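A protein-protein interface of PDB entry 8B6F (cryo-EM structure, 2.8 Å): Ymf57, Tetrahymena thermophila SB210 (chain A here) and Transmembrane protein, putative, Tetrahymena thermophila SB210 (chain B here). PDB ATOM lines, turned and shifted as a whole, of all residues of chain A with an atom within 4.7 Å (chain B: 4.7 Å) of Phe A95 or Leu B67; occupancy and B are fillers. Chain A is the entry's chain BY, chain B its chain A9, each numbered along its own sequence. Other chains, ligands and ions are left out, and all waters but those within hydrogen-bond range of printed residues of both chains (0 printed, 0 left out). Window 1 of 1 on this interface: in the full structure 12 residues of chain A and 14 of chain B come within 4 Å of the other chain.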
ATOM      1  N   PHE A  91      11.925  31.092 -22.109  1.00  0.00           N
ATOM      2  CA  PHE A  91      11.679  29.818 -21.445  1.00  0.00           C
ATOM      3  C   PHE A  91      10.792  28.910 -22.289  1.00  0.00           C
ATOM      4  O   PHE A  91      11.070  27.717 -22.437  1.00  0.00           O
ATOM      5  CB  PHE A  91      11.044  30.040 -20.075  1.00  0.00           C
ATOM      6  CG  PHE A  91      10.499  28.783 -19.465  1.00  0.00           C
ATOM      7  CD1 PHE A  91      11.335  27.913 -18.791  1.00  0.00           C
ATOM      8  CD2 PHE A  91       9.157  28.459 -19.588  1.00  0.00           C
ATOM      9  CE1 PHE A  91      10.847  26.748 -18.240  1.00  0.00           C
ATOM     10  CE2 PHE A  91       8.663  27.295 -19.038  1.00  0.00           C
ATOM     11  CZ  PHE A  91       9.509  26.439 -18.362  1.00  0.00           C
ATOM     12  N   ILE A  92       9.705  29.453 -22.839  1.00  0.00           N
ATOM     13  CA  ILE A  92       8.783  28.609 -23.591  1.00  0.00           C
ATOM     14  C   ILE A  92       9.420  28.140 -24.890  1.00  0.00           C
ATOM     15  O   ILE A  92       9.213  27.002 -25.324  1.00  0.00           O
ATOM     16  CB  ILE A  92       7.458  29.356 -23.839  1.00  0.00           C
ATOM     17  CG1 ILE A  92       6.315  28.362 -24.053  1.00  0.00           C
ATOM     18  CG2 ILE A  92       7.556  30.303 -25.034  1.00  0.00           C
ATOM     19  CD1 ILE A  92       5.897  27.625 -22.802  1.00  0.00           C
ATOM     20  N   THR A  93      10.198  29.005 -25.536  1.00  0.00           N
ATOM     21  CA  THR A  93      10.883  28.601 -26.756  1.00  0.00           C
ATOM     22  C   THR A  93      11.920  27.521 -26.480  1.00  0.00           C
ATOM     23  O   THR A  93      12.056  26.571 -27.258  1.00  0.00           O
ATOM     24  CB  THR A  93      11.522  29.821 -27.404  1.00  0.00           C
ATOM     25  OG1 THR A  93      12.247  30.545 -26.404  1.00  0.00           O
ATOM     26  CG2 THR A  93      10.461  30.713 -28.022  1.00  0.00           C
ATOM     27  N   ILE A  94      12.668  27.648 -25.380  1.00  0.00           N
ATOM     28  CA  ILE A  94      13.652  26.622 -25.052  1.00  0.00           C
ATOM     29  C   ILE A  94      12.950  25.331 -24.661  1.00  0.00           C
ATOM     30  O   ILE A  94      13.444  24.235 -24.947  1.00  0.00           O
ATOM     31  CB  ILE A  94      14.611  27.120 -23.949  1.00  0.00           C
ATOM     32  CG1 ILE A  94      16.027  26.589 -24.188  1.00  0.00           C
ATOM     33  CG2 ILE A  94      14.154  26.689 -22.561  1.00  0.00           C
ATOM     34  CD1 ILE A  94      16.730  27.199 -25.378  1.00  0.00           C
ATOM     35  N   PHE A  95      11.796  25.434 -24.001  1.00  0.00           N
ATOM     36  CA  PHE A  95      11.022  24.241 -23.685  1.00  0.00           C
ATOM     37  C   PHE A  95      10.568  23.537 -24.957  1.00  0.00           C
ATOM     38  O   PHE A  95      10.615  22.306 -25.047  1.00  0.00           O
ATOM     39  CB  PHE A  95       9.823  24.620 -22.814  1.00  0.00           C
ATOM     40  CG  PHE A  95       8.960  23.457 -22.434  1.00  0.00           C
ATOM     41  CD1 PHE A  95       9.222  22.726 -21.289  1.00  0.00           C
ATOM     42  CD2 PHE A  95       7.882  23.096 -23.224  1.00  0.00           C
ATOM     43  CE1 PHE A  95       8.425  21.656 -20.939  1.00  0.00           C
ATOM     44  CE2 PHE A  95       7.081  22.027 -22.880  1.00  0.00           C
ATOM     45  CZ  PHE A  95       7.352  21.307 -21.736  1.00  0.00           C
ATOM     46  N   ILE A  96      10.122  24.305 -25.951  1.00  0.00           N
ATOM     47  CA  ILE A  96       9.768  23.716 -27.239  1.00  0.00           C
ATOM     48  C   ILE A  96      10.997  23.095 -27.885  1.00  0.00           C
ATOM     49  O   ILE A  96      10.930  22.009 -28.470  1.00  0.00           O
ATOM     50  CB  ILE A  96       9.116  24.776 -28.148  1.00  0.00           C
ATOM     51  CG1 ILE A  96       7.732  25.149 -27.609  1.00  0.00           C
ATOM     52  CG2 ILE A  96       9.011  24.271 -29.586  1.00  0.00           C
ATOM     53  CD1 ILE A  96       7.086  26.324 -28.315  1.00  0.00           C
ATOM     54  N   LEU A  97      12.141  23.778 -27.795  1.00  0.00           N
ATOM     55  CA  LEU A  97      13.354  23.276 -28.429  1.00  0.00           C
ATOM     56  C   LEU A  97      13.781  21.938 -27.838  1.00  0.00           C
ATOM     57  O   LEU A  97      14.157  21.019 -28.572  1.00  0.00           O
ATOM     58  CB  LEU A  97      14.477  24.303 -28.283  1.00  0.00           C
ATOM     59  CG  LEU A  97      15.833  23.942 -28.893  1.00  0.00           C
ATOM     60  CD1 LEU A  97      15.728  23.805 -30.404  1.00  0.00           C
ATOM     61  CD2 LEU A  97      16.869  24.986 -28.523  1.00  0.00           C
ATOM     62  N   PHE A  98      13.728  21.809 -26.513  1.00  0.00           N
ATOM     63  CA  PHE A  98      14.247  20.620 -25.847  1.00  0.00           C
ATOM     64  C   PHE A  98      13.205  19.517 -25.717  1.00  0.00           C
ATOM     65  O   PHE A  98      13.468  18.370 -26.090  1.00  0.00           O
ATOM     66  CB  PHE A  98      14.776  20.984 -24.455  1.00  0.00           C
ATOM     67  CG  PHE A  98      16.070  21.755 -24.463  1.00  0.00           C
ATOM     68  CD1 PHE A  98      16.756  22.006 -25.643  1.00  0.00           C
ATOM     69  CD2 PHE A  98      16.606  22.221 -23.275  1.00  0.00           C
ATOM     70  CE1 PHE A  98      17.942  22.711 -25.632  1.00  0.00           C
ATOM     71  CE2 PHE A  98      17.789  22.925 -23.261  1.00  0.00           C
ATOM     72  CZ  PHE A  98      18.459  23.170 -24.439  1.00  0.00           C
ATOM     73  N   TYR A  99      12.026  19.840 -25.192  1.00  0.00           N
ATOM     74  CA  TYR A  99      11.090  18.825 -24.717  1.00  0.00           C
ATOM     75  C   TYR A  99      11.803  17.906 -23.727  1.00  0.00           C
ATOM     76  O   TYR A  99      11.991  16.710 -23.953  1.00  0.00           O
ATOM     77  CB  TYR A  99      10.481  18.034 -25.878  1.00  0.00           C
ATOM     78  CG  TYR A  99       9.333  18.744 -26.556  1.00  0.00           C
ATOM     79  CD1 TYR A  99       8.123  18.928 -25.899  1.00  0.00           C
ATOM     80  CD2 TYR A  99       9.453  19.214 -27.854  1.00  0.00           C
ATOM     81  CE1 TYR A  99       7.068  19.572 -26.515  1.00  0.00           C
ATOM     82  CE2 TYR A  99       8.403  19.857 -28.478  1.00  0.00           C
ATOM     83  CZ  TYR A  99       7.213  20.033 -27.803  1.00  0.00           C
ATOM     84  OH  TYR A  99       6.165  20.672 -28.420  1.00  0.00           O
ATOM     85  N   LYS B  63       7.144  17.048 -17.497  1.00  0.00           N
ATOM     86  CA  LYS B  63       6.839  18.187 -18.358  1.00  0.00           C
ATOM     87  C   LYS B  63       5.727  19.037 -17.759  1.00  0.00           C
ATOM     88  O   LYS B  63       5.825  20.268 -17.714  1.00  0.00           O
ATOM     89  CB  LYS B  63       6.447  17.698 -19.750  1.00  0.00           C
ATOM     90  CG  LYS B  63       7.624  17.340 -20.632  1.00  0.00           C
ATOM     91  CD  LYS B  63       7.159  16.706 -21.931  1.00  0.00           C
ATOM     92  CE  LYS B  63       8.298  16.593 -22.922  1.00  0.00           C
ATOM     93  NZ  LYS B  63       9.527  16.051 -22.286  1.00  0.00           N
ATOM     94  N   GLY B  64       4.653  18.394 -17.299  1.00  0.00           N
ATOM     95  CA  GLY B  64       3.557  19.138 -16.703  1.00  0.00           C
ATOM     96  C   GLY B  64       3.971  19.872 -15.443  1.00  0.00           C
ATOM     97  O   GLY B  64       3.559  21.011 -15.213  1.00  0.00           O
ATOM     98  N   ALA B  65       4.785  19.227 -14.606  1.00  0.00           N
ATOM     99  CA  ALA B  65       5.256  19.874 -13.386  1.00  0.00           C
ATOM    100  C   ALA B  65       6.134  21.076 -13.702  1.00  0.00           C
ATOM    101  O   ALA B  65       6.024  22.123 -13.055  1.00  0.00           O
ATOM    102  CB  ALA B  65       6.018  18.872 -12.521  1.00  0.00           C
ATOM    103  N   LEU B  66       7.011  20.947 -14.698  1.00  0.00           N
ATOM    104  CA  LEU B  66       7.847  22.075 -15.093  1.00  0.00           C
ATOM    105  C   LEU B  66       7.000  23.225 -15.620  1.00  0.00           C
ATOM    106  O   LEU B  66       7.266  24.393 -15.315  1.00  0.00           O
ATOM    107  CB  LEU B  66       8.864  21.629 -16.142  1.00  0.00           C
ATOM    108  CG  LEU B  66       9.794  22.712 -16.690  1.00  0.00           C
ATOM    109  CD1 LEU B  66      10.595  23.367 -15.576  1.00  0.00           C
ATOM    110  CD2 LEU B  66      10.718  22.125 -17.736  1.00  0.00           C
ATOM    111  N   LEU B  67       5.979  22.916 -16.419  1.00  0.00           N
ATOM    112  CA  LEU B  67       5.087  23.959 -16.914  1.00  0.00           C
ATOM    113  C   LEU B  67       4.359  24.647 -15.767  1.00  0.00           C
ATOM    114  O   LEU B  67       4.212  25.873 -15.763  1.00  0.00           O
ATOM    115  CB  LEU B  67       4.084  23.369 -17.904  1.00  0.00           C
ATOM    116  CG  LEU B  67       4.351  23.659 -19.381  1.00  0.00           C
ATOM    117  CD1 LEU B  67       5.749  23.229 -19.773  1.00  0.00           C
ATOM    118  CD2 LEU B  67       3.317  22.973 -20.252  1.00  0.00           C
ATOM    119  N   GLY B  68       3.883  23.871 -14.792  1.00  0.00           N
ATOM    120  CA  GLY B  68       3.209  24.470 -13.653  1.00  0.00           C
ATOM    121  C   GLY B  68       4.129  25.348 -12.829  1.00  0.00           C
ATOM    122  O   GLY B  68       3.734  26.424 -12.374  1.00  0.00           O
ATOM    123  N   VAL B  69       5.367  24.901 -12.620  1.00  0.00           N
ATOM    124  CA  VAL B  69       6.329  25.703 -11.871  1.00  0.00           C
ATOM    125  C   VAL B  69       6.639  26.992 -12.618  1.00  0.00           C
ATOM    126  O   VAL B  69       6.757  28.065 -12.013  1.00  0.00           O
ATOM    127  CB  VAL B  69       7.603  24.882 -11.592  1.00  0.00           C
ATOM    128  CG1 VAL B  69       8.723  25.771 -11.067  1.00  0.00           C
ATOM    129  CG2 VAL B  69       7.305  23.772 -10.598  1.00  0.00           C
ATOM    130  N   ALA B  70       6.777  26.913 -13.942  1.00  0.00           N
ATOM    131  CA  ALA B  70       7.014  28.118 -14.731  1.00  0.00           C
ATOM    132  C   ALA B  70       5.835  29.076 -14.636  1.00  0.00           C
ATOM    133  O   ALA B  70       6.023  30.290 -14.506  1.00  0.00           O
ATOM    134  CB  ALA B  70       7.285  27.746 -16.186  1.00  0.00           C
ATOM    135  N   TYR B  71       4.612  28.552 -14.708  1.00  0.00           N
ATOM    136  CA  TYR B  71       3.443  29.412 -14.568  1.00  0.00           C
ATOM    137  C   TYR B  71       3.419  30.076 -13.198  1.00  0.00           C
ATOM    138  O   TYR B  71       3.108  31.266 -13.080  1.00  0.00           O
ATOM    139  CB  TYR B  71       2.165  28.604 -14.796  1.00  0.00           C
ATOM    140  CG  TYR B  71       0.906  29.397 -14.540  1.00  0.00           C
ATOM    141  CD1 TYR B  71       0.424  30.293 -15.482  1.00  0.00           C
ATOM    142  CD2 TYR B  71       0.202  29.246 -13.354  1.00  0.00           C
ATOM    143  CE1 TYR B  71      -0.725  31.021 -15.249  1.00  0.00           C
ATOM    144  CE2 TYR B  71      -0.947  29.969 -13.111  1.00  0.00           C
ATOM    145  CZ  TYR B  71      -1.406  30.855 -14.063  1.00  0.00           C
ATOM    146  OH  TYR B  71      -2.550  31.577 -13.825  1.00  0.00           O
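The backbone carbonyl oxygen of Tyr A99 is in hydrogen-bond range of the side-chain amino group of Lys B63.
Among the printed residues, pairs that only touch across the chains: Phe A91 with Ala B70, Phe A95 with Leu B66 and Phe A95 with Leu B67.
Of chain B, only Leu B66 and Leu B67 come within 4 Å of Phe A95. Of the printed residues of chain A, Leu B67 touches Phe A95. Printed residues of chain A within 4 Å of Ala B70: Phe A91. Of the printed residues of chain A, Leu B66 touches Phe A95 (3.9 Å). The nearest residue of chain B that does not touch Phe A95 is Lys B63 (4.1 Å). The nearest printed residue of chain A that does not touch Leu B67 is Phe A91 (5.1 Å).
Hydrophobic or aromatic side chains of chain B within 4 Å of the printed part of chain A: Leu B66, Leu B67 and Ala B70. Printed residues of chain A that touch a printed residue of chain B: Phe A91, Phe A95 and Tyr A99. Among the printed residues, no Asp or Glu carboxylate lies within 4 Å of a Lys or Arg side-chain nitrogen of the other chain.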
